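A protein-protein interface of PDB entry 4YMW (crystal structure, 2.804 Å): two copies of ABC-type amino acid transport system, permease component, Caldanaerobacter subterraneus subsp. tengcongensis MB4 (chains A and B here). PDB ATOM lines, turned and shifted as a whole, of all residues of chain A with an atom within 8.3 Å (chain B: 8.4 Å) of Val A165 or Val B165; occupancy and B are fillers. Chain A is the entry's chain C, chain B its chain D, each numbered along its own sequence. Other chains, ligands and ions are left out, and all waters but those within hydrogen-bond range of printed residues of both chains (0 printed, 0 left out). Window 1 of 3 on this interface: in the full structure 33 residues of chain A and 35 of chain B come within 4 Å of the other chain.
The side-chain hydroxyl (OG) of Ser B164 is in hydrogen-bond range of the backbone carbonyl oxygen (O) of Ala B161, 3.3 Å away.
The backbone carbonyl oxygen (O) of Ala A161 sits at hydrogen-bond distance from the side-chain hydroxyl (OG) of Ser A164 (3.3 Å).
Ala B161 touches Leu A68 (O to CD2, 3.2 Å).
Leu A68 touches Ile B162.
Ser B164 touches Leu A68 (OG to CD2, 3.7 Å).
Leu A68 touches Val B165.
Ala A161 touches Leu B68.
Ile A162 touches Leu B68.
OG of Ser A164 touches CD2 of Leu B68 (3.6 Å).
Val B165 touches Val A165.
Val A165 touches just one residue of chain B: Val B165 (3.7 Å).
Of chain A, only Leu A68 (3.96 Å) and Val A165 (3.7 Å) come within 4 Å of Val B165.
Of chain B, only Leu B68 (3.6 Å) comes within 4 Å of Ser A164.
Ser B164 touches one residue of chain A.
Printed residues of chain A within 4 Å of Ile B162: Leu A68.
Printed residues of chain A within 4 Å of Leu B68: Ala A161, Ile A162 and Ser A164.
Of the printed residues of chain B, Ala A161 touches Leu B68 (3.1 Å).
Printed residues of chain B within 4 Å of Leu A68: Ala B161, Ile B162, Ser B164 and Val B165.
Ser A160 touches none of the printed residues of chain B.
The nearest residue of chain B that does not touch Val A165 is Leu B68 (4.1 Å).
Of the 20 printed residues of chain B, 5 touch a printed residue of chain A.
Hydrophobic or aromatic side chains of chain B that line the printed part of chain A: Leu B68 and Val B165.
Hydrophobic or aromatic side chains of chain A within 4 Å of the printed part of chain B: Leu A68 and Val A165.
Among the printed residues, 8 pairs touch across the chains.
Leu A68 touches Ala B161, and with the chains exchanged Ala A161 touches Leu B68.
Leu A68 touches Ile B162, and with the chains exchanged Ile A162 touches Leu B68.
Leu A68 touches Ser B164, and with the chains exchanged Ser A164 touches Leu B68.
Val A165 touches its own counterpart, Val B165.
Positions printed for both chains: 68, 71, 72, 75, 76, 87, 160, 161, 162, 163, 164, 165, 166, 167, 168, 169, 170, 172, 173 and 176.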
ATOM      1  N   LEU A  68     -13.712  13.291  -6.319  1.00  0.00           N
ATOM      2  CA  LEU A  68     -14.789  13.037  -7.270  1.00  0.00           C
ATOM      3  C   LEU A  68     -16.030  13.851  -6.920  1.00  0.00           C
ATOM      4  O   LEU A  68     -16.589  14.530  -7.788  1.00  0.00           O
ATOM      5  CB  LEU A  68     -15.141  11.557  -7.332  1.00  0.00           C
ATOM      6  CG  LEU A  68     -16.328  11.225  -8.238  1.00  0.00           C
ATOM      7  CD1 LEU A  68     -16.050  11.696  -9.640  1.00  0.00           C
ATOM      8  CD2 LEU A  68     -16.562   9.732  -8.252  1.00  0.00           C
ATOM      9  N   LEU A  71     -15.691  17.465  -7.758  1.00  0.00           N
ATOM     10  CA  LEU A  71     -15.850  17.633  -9.201  1.00  0.00           C
ATOM     11  C   LEU A  71     -17.343  17.658  -9.551  1.00  0.00           C
ATOM     12  O   LEU A  71     -17.821  18.577 -10.222  1.00  0.00           O
ATOM     13  CB  LEU A  71     -15.117  16.529  -9.976  1.00  0.00           C
ATOM     14  CG  LEU A  71     -15.240  16.622 -11.498  1.00  0.00           C
ATOM     15  CD1 LEU A  71     -14.461  17.812 -12.054  1.00  0.00           C
ATOM     16  CD2 LEU A  71     -14.713  15.354 -12.101  1.00  0.00           C
ATOM     17  N   LEU A  72     -18.075  16.658  -9.072  1.00  0.00           N
ATOM     18  CA  LEU A  72     -19.513  16.601  -9.271  1.00  0.00           C
ATOM     19  C   LEU A  72     -20.242  17.790  -8.634  1.00  0.00           C
ATOM     20  O   LEU A  72     -21.292  18.181  -9.115  1.00  0.00           O
ATOM     21  CB  LEU A  72     -20.070  15.261  -8.790  1.00  0.00           C
ATOM     22  CG  LEU A  72     -19.415  14.120  -9.595  1.00  0.00           C
ATOM     23  CD1 LEU A  72     -20.023  12.742  -9.358  1.00  0.00           C
ATOM     24  CD2 LEU A  72     -19.392  14.434 -11.085  1.00  0.00           C
ATOM     25  N   TYR A  75     -19.649  20.512 -11.351  1.00  0.00           N
ATOM     26  CA  TYR A  75     -20.308  20.251 -12.628  1.00  0.00           C
ATOM     27  C   TYR A  75     -21.838  20.152 -12.476  1.00  0.00           C
ATOM     28  O   TYR A  75     -22.572  21.040 -12.906  1.00  0.00           O
ATOM     29  CB  TYR A  75     -19.737  18.973 -13.243  1.00  0.00           C
ATOM     30  CG  TYR A  75     -19.943  18.790 -14.739  1.00  0.00           C
ATOM     31  CD1 TYR A  75     -20.700  17.737 -15.236  1.00  0.00           C
ATOM     32  CD2 TYR A  75     -19.313  19.630 -15.652  1.00  0.00           C
ATOM     33  CE1 TYR A  75     -20.858  17.549 -16.602  1.00  0.00           C
ATOM     34  CE2 TYR A  75     -19.460  19.453 -17.013  1.00  0.00           C
ATOM     35  CZ  TYR A  75     -20.243  18.413 -17.491  1.00  0.00           C
ATOM     36  OH  TYR A  75     -20.400  18.242 -18.858  1.00  0.00           O
ATOM     37  N   ASN A  76     -22.311  19.074 -11.860  1.00  0.00           N
ATOM     38  CA  ASN A  76     -23.741  18.819 -11.699  1.00  0.00           C
ATOM     39  C   ASN A  76     -24.503  19.640 -10.662  1.00  0.00           C
ATOM     40  O   ASN A  76     -25.591  20.139 -10.932  1.00  0.00           O
ATOM     41  CB  ASN A  76     -23.929  17.360 -11.357  1.00  0.00           C
ATOM     42  CG  ASN A  76     -23.357  16.468 -12.405  1.00  0.00           C
ATOM     43  OD1 ASN A  76     -22.969  16.933 -13.475  1.00  0.00           O
ATOM     44  ND2 ASN A  76     -23.296  15.174 -12.117  1.00  0.00           N
ATOM     45  N   ALA A  87     -16.871  21.125 -19.271  1.00  0.00           N
ATOM     46  CA  ALA A  87     -16.255  20.061 -18.483  1.00  0.00           C
ATOM     47  C   ALA A  87     -14.858  20.478 -18.043  1.00  0.00           C
ATOM     48  O   ALA A  87     -14.424  20.180 -16.933  1.00  0.00           O
ATOM     49  CB  ALA A  87     -16.195  18.787 -19.271  1.00  0.00           C
ATOM     50  N   SER A 160      -5.916  13.409 -12.201  1.00  0.00           N
ATOM     51  CA  SER A 160      -6.638  14.142 -13.230  1.00  0.00           C
ATOM     52  C   SER A 160      -7.404  13.229 -14.194  1.00  0.00           C
ATOM     53  O   SER A 160      -8.320  13.665 -14.891  1.00  0.00           O
ATOM     54  CB  SER A 160      -5.664  15.029 -14.002  1.00  0.00           C
ATOM     55  OG  SER A 160      -4.759  14.242 -14.759  1.00  0.00           O
ATOM     56  N   ALA A 161      -7.038  11.957 -14.229  1.00  0.00           N
ATOM     57  CA  ALA A 161      -7.774  10.994 -15.026  1.00  0.00           C
ATOM     58  C   ALA A 161      -9.241  10.922 -14.624  1.00  0.00           C
ATOM     59  O   ALA A 161     -10.028  10.310 -15.334  1.00  0.00           O
ATOM     60  CB  ALA A 161      -7.147   9.609 -14.915  1.00  0.00           C
ATOM     61  N   ILE A 162      -9.629  11.524 -13.500  1.00  0.00           N
ATOM     62  CA  ILE A 162     -11.016  11.369 -13.092  1.00  0.00           C
ATOM     63  C   ILE A 162     -11.936  12.378 -13.781  1.00  0.00           C
ATOM     64  O   ILE A 162     -13.159  12.246 -13.695  1.00  0.00           O
ATOM     65  CB  ILE A 162     -11.207  11.456 -11.571  1.00  0.00           C
ATOM     66  CG1 ILE A 162     -12.319  10.487 -11.157  1.00  0.00           C
ATOM     67  CG2 ILE A 162     -11.444  12.886 -11.114  1.00  0.00           C
ATOM     68  CD1 ILE A 162     -12.760  10.615  -9.752  1.00  0.00           C
ATOM     69  N   VAL A 163     -11.382  13.372 -14.477  1.00  0.00           N
ATOM     70  CA  VAL A 163     -12.255  14.290 -15.214  1.00  0.00           C
ATOM     71  C   VAL A 163     -12.756  13.606 -16.479  1.00  0.00           C
ATOM     72  O   VAL A 163     -13.522  14.191 -17.241  1.00  0.00           O
ATOM     73  CB  VAL A 163     -11.570  15.614 -15.632  1.00  0.00           C
ATOM     74  CG1 VAL A 163     -11.023  16.354 -14.432  1.00  0.00           C
ATOM     75  CG2 VAL A 163     -10.495  15.357 -16.682  1.00  0.00           C
ATOM     76  N   SER A 164     -12.316  12.372 -16.716  1.00  0.00           N
ATOM     77  CA  SER A 164     -12.805  11.629 -17.862  1.00  0.00           C
ATOM     78  C   SER A 164     -14.272  11.341 -17.619  1.00  0.00           C
ATOM     79  O   SER A 164     -15.074  11.458 -18.539  1.00  0.00           O
ATOM     80  CB  SER A 164     -12.046  10.335 -18.067  1.00  0.00           C
ATOM     81  OG  SER A 164     -12.556   9.350 -17.196  1.00  0.00           O
ATOM     82  N   VAL A 165     -14.639  10.993 -16.384  1.00  0.00           N
ATOM     83  CA  VAL A 165     -16.037  10.664 -16.076  1.00  0.00           C
ATOM     84  C   VAL A 165     -16.996  11.840 -16.331  1.00  0.00           C
ATOM     85  O   VAL A 165     -18.211  11.685 -16.258  1.00  0.00           O
ATOM     86  CB  VAL A 165     -16.229  10.198 -14.612  1.00  0.00           C
ATOM     87  CG1 VAL A 165     -15.144   9.226 -14.220  1.00  0.00           C
ATOM     88  CG2 VAL A 165     -16.261  11.376 -13.670  1.00  0.00           C
ATOM     89  N   ILE A 166     -16.441  13.011 -16.625  1.00  0.00           N
ATOM     90  CA  ILE A 166     -17.212  14.221 -16.882  1.00  0.00           C
ATOM     91  C   ILE A 166     -17.227  14.478 -18.404  1.00  0.00           C
ATOM     92  O   ILE A 166     -17.813  15.443 -18.891  1.00  0.00           O
ATOM     93  CB  ILE A 166     -16.579  15.423 -16.102  1.00  0.00           C
ATOM     94  CG1 ILE A 166     -17.604  16.349 -15.481  1.00  0.00           C
ATOM     95  CG2 ILE A 166     -15.590  16.236 -16.946  1.00  0.00           C
ATOM     96  CD1 ILE A 166     -16.912  17.465 -14.745  1.00  0.00           C
ATOM     97  N   GLY A 167     -16.562  13.597 -19.151  1.00  0.00           N
ATOM     98  CA  GLY A 167     -16.492  13.686 -20.600  1.00  0.00           C
ATOM     99  C   GLY A 167     -15.433  14.611 -21.181  1.00  0.00           C
ATOM    100  O   GLY A 167     -15.534  15.022 -22.333  1.00  0.00           O
ATOM    101  N   PHE A 168     -14.405  14.927 -20.402  1.00  0.00           N
ATOM    102  CA  PHE A 168     -13.261  15.690 -20.902  1.00  0.00           C
ATOM    103  C   PHE A 168     -12.331  14.748 -21.660  1.00  0.00           C
ATOM    104  O   PHE A 168     -12.131  13.598 -21.258  1.00  0.00           O
ATOM    105  CB  PHE A 168     -12.545  16.384 -19.743  1.00  0.00           C
ATOM    106  CG  PHE A 168     -11.351  17.216 -20.154  1.00  0.00           C
ATOM    107  CD1 PHE A 168     -11.518  18.468 -20.735  1.00  0.00           C
ATOM    108  CD2 PHE A 168     -10.050  16.757 -19.914  1.00  0.00           C
ATOM    109  CE1 PHE A 168     -10.415  19.234 -21.104  1.00  0.00           C
ATOM    110  CE2 PHE A 168      -8.946  17.514 -20.277  1.00  0.00           C
ATOM    111  CZ  PHE A 168      -9.128  18.756 -20.870  1.00  0.00           C
ATOM    112  N   ALA A 169     -11.777  15.228 -22.768  1.00  0.00           N
ATOM    113  CA  ALA A 169     -11.033  14.364 -23.684  1.00  0.00           C
ATOM    114  C   ALA A 169      -9.568  14.210 -23.298  1.00  0.00           C
ATOM    115  O   ALA A 169      -8.675  14.524 -24.092  1.00  0.00           O
ATOM    116  CB  ALA A 169     -11.143  14.898 -25.103  1.00  0.00           C
ATOM    117  N   ASP A 170      -9.334  13.751 -22.070  1.00  0.00           N
ATOM    118  CA  ASP A 170      -7.989  13.516 -21.545  1.00  0.00           C
ATOM    119  C   ASP A 170      -7.452  12.151 -21.984  1.00  0.00           C
ATOM    120  O   ASP A 170      -8.006  11.516 -22.862  1.00  0.00           O
ATOM    121  CB  ASP A 170      -7.990  13.629 -20.019  1.00  0.00           C
ATOM    122  CG  ASP A 170      -8.635  12.427 -19.345  1.00  0.00           C
ATOM    123  OD1 ASP A 170      -9.630  11.909 -19.894  1.00  0.00           O
ATOM    124  OD2 ASP A 170      -8.157  12.000 -18.268  1.00  0.00           O
ATOM    125  N   THR A 172      -7.522   9.324 -20.484  1.00  0.00           N
ATOM    126  CA  THR A 172      -8.350   8.170 -20.120  1.00  0.00           C
ATOM    127  C   THR A 172      -9.623   8.024 -20.973  1.00  0.00           C
ATOM    128  O   THR A 172     -10.043   6.906 -21.286  1.00  0.00           O
ATOM    129  CB  THR A 172      -8.694   8.228 -18.618  1.00  0.00           C
ATOM    130  OG1 THR A 172      -7.492   7.994 -17.886  1.00  0.00           O
ATOM    131  CG2 THR A 172      -9.670   7.148 -18.213  1.00  0.00           C
ATOM    132  N   ARG A 173     -10.211   9.143 -21.378  1.00  0.00           N
ATOM    133  CA  ARG A 173     -11.414   9.133 -22.218  1.00  0.00           C
ATOM    134  C   ARG A 173     -11.153   8.462 -23.572  1.00  0.00           C
ATOM    135  O   ARG A 173     -12.055   7.842 -24.169  1.00  0.00           O
ATOM    136  CB  ARG A 173     -11.929  10.568 -22.393  1.00  0.00           C
ATOM    137  CG  ARG A 173     -13.333  10.715 -22.968  1.00  0.00           C
ATOM    138  CD  ARG A 173     -14.422   9.991 -22.145  1.00  0.00           C
ATOM    139  NE  ARG A 173     -15.773  10.481 -22.448  1.00  0.00           N
ATOM    140  CZ  ARG A 173     -16.357  10.456 -23.644  1.00  0.00           C
ATOM    141  NH1 ARG A 173     -15.730   9.966 -24.710  1.00  0.00           N
ATOM    142  NH2 ARG A 173     -17.581  10.949 -23.783  1.00  0.00           N
ATOM    143  N   ASP A 176     -12.661   5.172 -24.243  1.00  0.00           N
ATOM    144  CA  ASP A 176     -14.059   5.213 -24.665  1.00  0.00           C
ATOM    145  C   ASP A 176     -14.110   5.530 -26.150  1.00  0.00           C
ATOM    146  O   ASP A 176     -14.685   4.751 -26.938  1.00  0.00           O
ATOM    147  CB  ASP A 176     -14.876   6.223 -23.845  1.00  0.00           C
ATOM    148  CG  ASP A 176     -15.298   5.666 -22.479  1.00  0.00           C
ATOM    149  OD1 ASP A 176     -15.421   4.426 -22.356  1.00  0.00           O
ATOM    150  OD2 ASP A 176     -15.515   6.458 -21.534  1.00  0.00           O
ATOM    151  N   LEU B  68      -8.514   4.841 -11.377  1.00  0.00           N
ATOM    152  CA  LEU B  68      -9.643   4.809 -12.294  1.00  0.00           C
ATOM    153  C   LEU B  68      -9.377   3.864 -13.461  1.00  0.00           C
ATOM    154  O   LEU B  68     -10.196   2.975 -13.747  1.00  0.00           O
ATOM    155  CB  LEU B  68      -9.953   6.213 -12.804  1.00  0.00           C
ATOM    156  CG  LEU B  68     -11.091   6.281 -13.813  1.00  0.00           C
ATOM    157  CD1 LEU B  68     -12.346   5.750 -13.178  1.00  0.00           C
ATOM    158  CD2 LEU B  68     -11.321   7.701 -14.288  1.00  0.00           C
ATOM    159  N   LEU B  71      -9.695   0.281 -12.431  1.00  0.00           N
ATOM    160  CA  LEU B  71     -11.085  -0.115 -12.255  1.00  0.00           C
ATOM    161  C   LEU B  71     -11.686  -0.460 -13.619  1.00  0.00           C
ATOM    162  O   LEU B  71     -12.180  -1.581 -13.841  1.00  0.00           O
ATOM    163  CB  LEU B  71     -11.889   1.011 -11.584  1.00  0.00           C
ATOM    164  CG  LEU B  71     -13.381   0.810 -11.290  1.00  0.00           C
ATOM    165  CD1 LEU B  71     -13.557  -0.141 -10.126  1.00  0.00           C
ATOM    166  CD2 LEU B  71     -14.087   2.112 -10.998  1.00  0.00           C
ATOM    167  N   LEU B  72     -11.576   0.490 -14.549  1.00  0.00           N
ATOM    168  CA  LEU B  72     -12.087   0.305 -15.908  1.00  0.00           C
ATOM    169  C   LEU B  72     -11.419  -0.870 -16.639  1.00  0.00           C
ATOM    170  O   LEU B  72     -12.084  -1.573 -17.381  1.00  0.00           O
ATOM    171  CB  LEU B  72     -11.911   1.596 -16.713  1.00  0.00           C
ATOM    172  CG  LEU B  72     -12.614   2.809 -16.086  1.00  0.00           C
ATOM    173  CD1 LEU B  72     -12.561   4.057 -16.964  1.00  0.00           C
ATOM    174  CD2 LEU B  72     -14.057   2.483 -15.697  1.00  0.00           C
ATOM    175  N   TYR B  75     -13.189  -3.871 -15.358  1.00  0.00           N
ATOM    176  CA  TYR B  75     -14.604  -3.851 -15.783  1.00  0.00           C
ATOM    177  C   TYR B  75     -14.823  -3.955 -17.307  1.00  0.00           C
ATOM    178  O   TYR B  75     -15.247  -4.986 -17.830  1.00  0.00           O
ATOM    179  CB  TYR B  75     -15.244  -2.560 -15.275  1.00  0.00           C
ATOM    180  CG  TYR B  75     -16.754  -2.523 -15.231  1.00  0.00           C
ATOM    181  CD1 TYR B  75     -17.467  -1.675 -16.070  1.00  0.00           C
ATOM    182  CD2 TYR B  75     -17.469  -3.297 -14.321  1.00  0.00           C
ATOM    183  CE1 TYR B  75     -18.845  -1.603 -16.022  1.00  0.00           C
ATOM    184  CE2 TYR B  75     -18.855  -3.229 -14.261  1.00  0.00           C
ATOM    185  CZ  TYR B  75     -19.535  -2.378 -15.121  1.00  0.00           C
ATOM    186  OH  TYR B  75     -20.909  -2.308 -15.082  1.00  0.00           O
ATOM    187  N   ASN B  76     -14.502  -2.874 -18.001  1.00  0.00           N
ATOM    188  CA  ASN B  76     -14.659  -2.793 -19.439  1.00  0.00           C
ATOM    189  C   ASN B  76     -13.677  -3.660 -20.208  1.00  0.00           C
ATOM    190  O   ASN B  76     -14.044  -4.319 -21.172  1.00  0.00           O
ATOM    191  CB  ASN B  76     -14.522  -1.344 -19.890  1.00  0.00           C
ATOM    192  CG  ASN B  76     -15.616  -0.462 -19.334  1.00  0.00           C
ATOM    193  OD1 ASN B  76     -16.599  -0.957 -18.785  1.00  0.00           O
ATOM    194  ND2 ASN B  76     -15.465   0.850 -19.488  1.00  0.00           N
ATOM    195  N   ALA B  87     -20.579  -5.107 -10.992  1.00  0.00           N
ATOM    196  CA  ALA B  87     -19.928  -3.854 -10.620  1.00  0.00           C
ATOM    197  C   ALA B  87     -19.178  -3.985  -9.283  1.00  0.00           C
ATOM    198  O   ALA B  87     -18.070  -3.464  -9.118  1.00  0.00           O
ATOM    199  CB  ALA B  87     -20.946  -2.741 -10.540  1.00  0.00           C
ATOM    200  N   SER B 160     -12.859   5.050  -2.552  1.00  0.00           N
ATOM    201  CA  SER B 160     -13.864   4.103  -3.046  1.00  0.00           C
ATOM    202  C   SER B 160     -15.077   4.782  -3.705  1.00  0.00           C
ATOM    203  O   SER B 160     -15.830   4.146  -4.446  1.00  0.00           O
ATOM    204  CB  SER B 160     -14.353   3.198  -1.916  1.00  0.00           C
ATOM    205  OG  SER B 160     -15.138   3.919  -0.988  1.00  0.00           O
ATOM    206  N   ALA B 161     -15.257   6.077  -3.454  1.00  0.00           N
ATOM    207  CA  ALA B 161     -16.320   6.848  -4.100  1.00  0.00           C
ATOM    208  C   ALA B 161     -16.229   6.780  -5.628  1.00  0.00           C
ATOM    209  O   ALA B 161     -17.123   7.248  -6.329  1.00  0.00           O
ATOM    210  CB  ALA B 161     -16.284   8.317  -3.634  1.00  0.00           C
ATOM    211  N   ILE B 162     -15.142   6.224  -6.145  1.00  0.00           N
ATOM    212  CA  ILE B 162     -14.938   6.170  -7.578  1.00  0.00           C
ATOM    213  C   ILE B 162     -15.664   5.003  -8.235  1.00  0.00           C
ATOM    214  O   ILE B 162     -15.760   4.952  -9.456  1.00  0.00           O
ATOM    215  CB  ILE B 162     -13.453   6.073  -7.933  1.00  0.00           C
ATOM    216  CG1 ILE B 162     -13.216   6.647  -9.323  1.00  0.00           C
ATOM    217  CG2 ILE B 162     -12.968   4.633  -7.871  1.00  0.00           C
ATOM    218  CD1 ILE B 162     -11.864   6.356  -9.843  1.00  0.00           C
ATOM    219  N   VAL B 163     -16.186   4.067  -7.447  1.00  0.00           N
ATOM    220  CA  VAL B 163     -16.938   2.958  -8.038  1.00  0.00           C
ATOM    221  C   VAL B 163     -18.348   3.384  -8.445  1.00  0.00           C
ATOM    222  O   VAL B 163     -19.108   2.598  -9.004  1.00  0.00           O
ATOM    223  CB  VAL B 163     -17.060   1.766  -7.077  1.00  0.00           C
ATOM    224  CG1 VAL B 163     -15.689   1.306  -6.631  1.00  0.00           C
ATOM    225  CG2 VAL B 163     -17.953   2.133  -5.885  1.00  0.00           C
ATOM    226  N   SER B 164     -18.695   4.629  -8.151  1.00  0.00           N
ATOM    227  CA  SER B 164     -19.983   5.150  -8.541  1.00  0.00           C
ATOM    228  C   SER B 164     -20.043   5.291 -10.062  1.00  0.00           C
ATOM    229  O   SER B 164     -21.046   4.914 -10.690  1.00  0.00           O
ATOM    230  CB  SER B 164     -20.241   6.482  -7.855  1.00  0.00           C
ATOM    231  OG  SER B 164     -19.542   7.505  -8.524  1.00  0.00           O
ATOM    232  N   VAL B 165     -18.963   5.786 -10.668  1.00  0.00           N
ATOM    233  CA  VAL B 165     -18.954   6.011 -12.118  1.00  0.00           C
ATOM    234  C   VAL B 165     -19.140   4.715 -12.915  1.00  0.00           C
ATOM    235  O   VAL B 165     -19.307   4.737 -14.128  1.00  0.00           O
ATOM    236  CB  VAL B 165     -17.659   6.706 -12.575  1.00  0.00           C
ATOM    237  CG1 VAL B 165     -17.334   7.825 -11.640  1.00  0.00           C
ATOM    238  CG2 VAL B 165     -16.516   5.730 -12.646  1.00  0.00           C
ATOM    239  N   ILE B 166     -19.102   3.591 -12.216  1.00  0.00           N
ATOM    240  CA  ILE B 166     -19.254   2.275 -12.806  1.00  0.00           C
ATOM    241  C   ILE B 166     -20.661   1.764 -12.481  1.00  0.00           C
ATOM    242  O   ILE B 166     -21.027   0.622 -12.797  1.00  0.00           O
ATOM    243  CB  ILE B 166     -18.171   1.317 -12.263  1.00  0.00           C
ATOM    244  CG1 ILE B 166     -17.644   0.385 -13.329  1.00  0.00           C
ATOM    245  CG2 ILE B 166     -18.644   0.507 -11.042  1.00  0.00           C
ATOM    246  CD1 ILE B 166     -16.576  -0.508 -12.740  1.00  0.00           C
ATOM    247  N   GLY B 167     -21.427   2.604 -11.789  1.00  0.00           N
ATOM    248  CA  GLY B 167     -22.787   2.258 -11.430  1.00  0.00           C
ATOM    249  C   GLY B 167     -22.971   1.398 -10.188  1.00  0.00           C
ATOM    250  O   GLY B 167     -23.960   0.672 -10.072  1.00  0.00           O
ATOM    251  N   PHE B 168     -21.998   1.410  -9.283  1.00  0.00           N
ATOM    252  CA  PHE B 168     -22.175   0.751  -7.990  1.00  0.00           C
ATOM    253  C   PHE B 168     -22.904   1.700  -7.035  1.00  0.00           C
ATOM    254  O   PHE B 168     -22.643   2.900  -7.046  1.00  0.00           O
ATOM    255  CB  PHE B 168     -20.836   0.327  -7.404  1.00  0.00           C
ATOM    256  CG  PHE B 168     -20.963  -0.453  -6.133  1.00  0.00           C
ATOM    257  CD1 PHE B 168     -21.309  -1.798  -6.167  1.00  0.00           C
ATOM    258  CD2 PHE B 168     -20.758   0.160  -4.900  1.00  0.00           C
ATOM    259  CE1 PHE B 168     -21.440  -2.525  -4.998  1.00  0.00           C
ATOM    260  CE2 PHE B 168     -20.886  -0.562  -3.722  1.00  0.00           C
ATOM    261  CZ  PHE B 168     -21.228  -1.909  -3.770  1.00  0.00           C
ATOM    262  N   ALA B 169     -23.808   1.176  -6.212  1.00  0.00           N
ATOM    263  CA  ALA B 169     -24.673   2.039  -5.399  1.00  0.00           C
ATOM    264  C   ALA B 169     -24.052   2.463  -4.064  1.00  0.00           C
ATOM    265  O   ALA B 169     -24.636   2.246  -2.996  1.00  0.00           O
ATOM    266  CB  ALA B 169     -26.000   1.350  -5.151  1.00  0.00           C
ATOM    267  N   ASP B 170     -22.879   3.091  -4.133  1.00  0.00           N
ATOM    268  CA  ASP B 170     -22.180   3.593  -2.952  1.00  0.00           C
ATOM    269  C   ASP B 170     -22.771   4.932  -2.527  1.00  0.00           C
ATOM    270  O   ASP B 170     -23.784   5.359  -3.065  1.00  0.00           O
ATOM    271  CB  ASP B 170     -20.688   3.749  -3.246  1.00  0.00           C
ATOM    272  CG  ASP B 170     -20.396   4.959  -4.126  1.00  0.00           C
ATOM    273  OD1 ASP B 170     -21.192   5.231  -5.050  1.00  0.00           O
ATOM    274  OD2 ASP B 170     -19.386   5.660  -3.885  1.00  0.00           O
ATOM    275  N   THR B 172     -21.860   7.908  -3.199  1.00  0.00           N
ATOM    276  CA  THR B 172     -21.829   8.979  -4.204  1.00  0.00           C
ATOM    277  C   THR B 172     -22.942   8.763  -5.251  1.00  0.00           C
ATOM    278  O   THR B 172     -23.507   9.720  -5.799  1.00  0.00           O
ATOM    279  CB  THR B 172     -20.446   9.077  -4.896  1.00  0.00           C
ATOM    280  OG1 THR B 172     -19.453   9.447  -3.934  1.00  0.00           O
ATOM    281  CG2 THR B 172     -20.464  10.133  -5.997  1.00  0.00           C
ATOM    282  N   ARG B 173     -23.264   7.498  -5.510  1.00  0.00           N
ATOM    283  CA  ARG B 173     -24.316   7.139  -6.458  1.00  0.00           C
ATOM    284  C   ARG B 173     -25.670   7.711  -6.024  1.00  0.00           C
ATOM    285  O   ARG B 173     -26.540   8.039  -6.855  1.00  0.00           O
ATOM    286  CB  ARG B 173     -24.414   5.616  -6.567  1.00  0.00           C
ATOM    287  CG  ARG B 173     -25.183   5.100  -7.763  1.00  0.00           C
ATOM    288  CD  ARG B 173     -24.491   5.517  -9.047  1.00  0.00           C
ATOM    289  NE  ARG B 173     -25.001   4.788 -10.202  1.00  0.00           N
ATOM    290  CZ  ARG B 173     -25.288   5.352 -11.371  1.00  0.00           C
ATOM    291  NH1 ARG B 173     -25.103   6.656 -11.549  1.00  0.00           N
ATOM    292  NH2 ARG B 173     -25.750   4.609 -12.366  1.00  0.00           N
ATOM    293  N   ASP B 176     -27.077  10.716  -7.799  1.00  0.00           N
ATOM    294  CA  ASP B 176     -27.704  10.417  -9.078  1.00  0.00           C
ATOM    295  C   ASP B 176     -29.123   9.947  -8.826  1.00  0.00           C
ATOM    296  O   ASP B 176     -30.096  10.545  -9.324  1.00  0.00           O
ATOM    297  CB  ASP B 176     -26.952   9.332  -9.866  1.00  0.00           C
ATOM    298  CG  ASP B 176     -25.698   9.851 -10.549  1.00  0.00           C
ATOM    299  OD1 ASP B 176     -25.605  11.079 -10.813  1.00  0.00           O
ATOM    300  OD2 ASP B 176     -24.833   9.007 -10.878  1.00  0.00           O
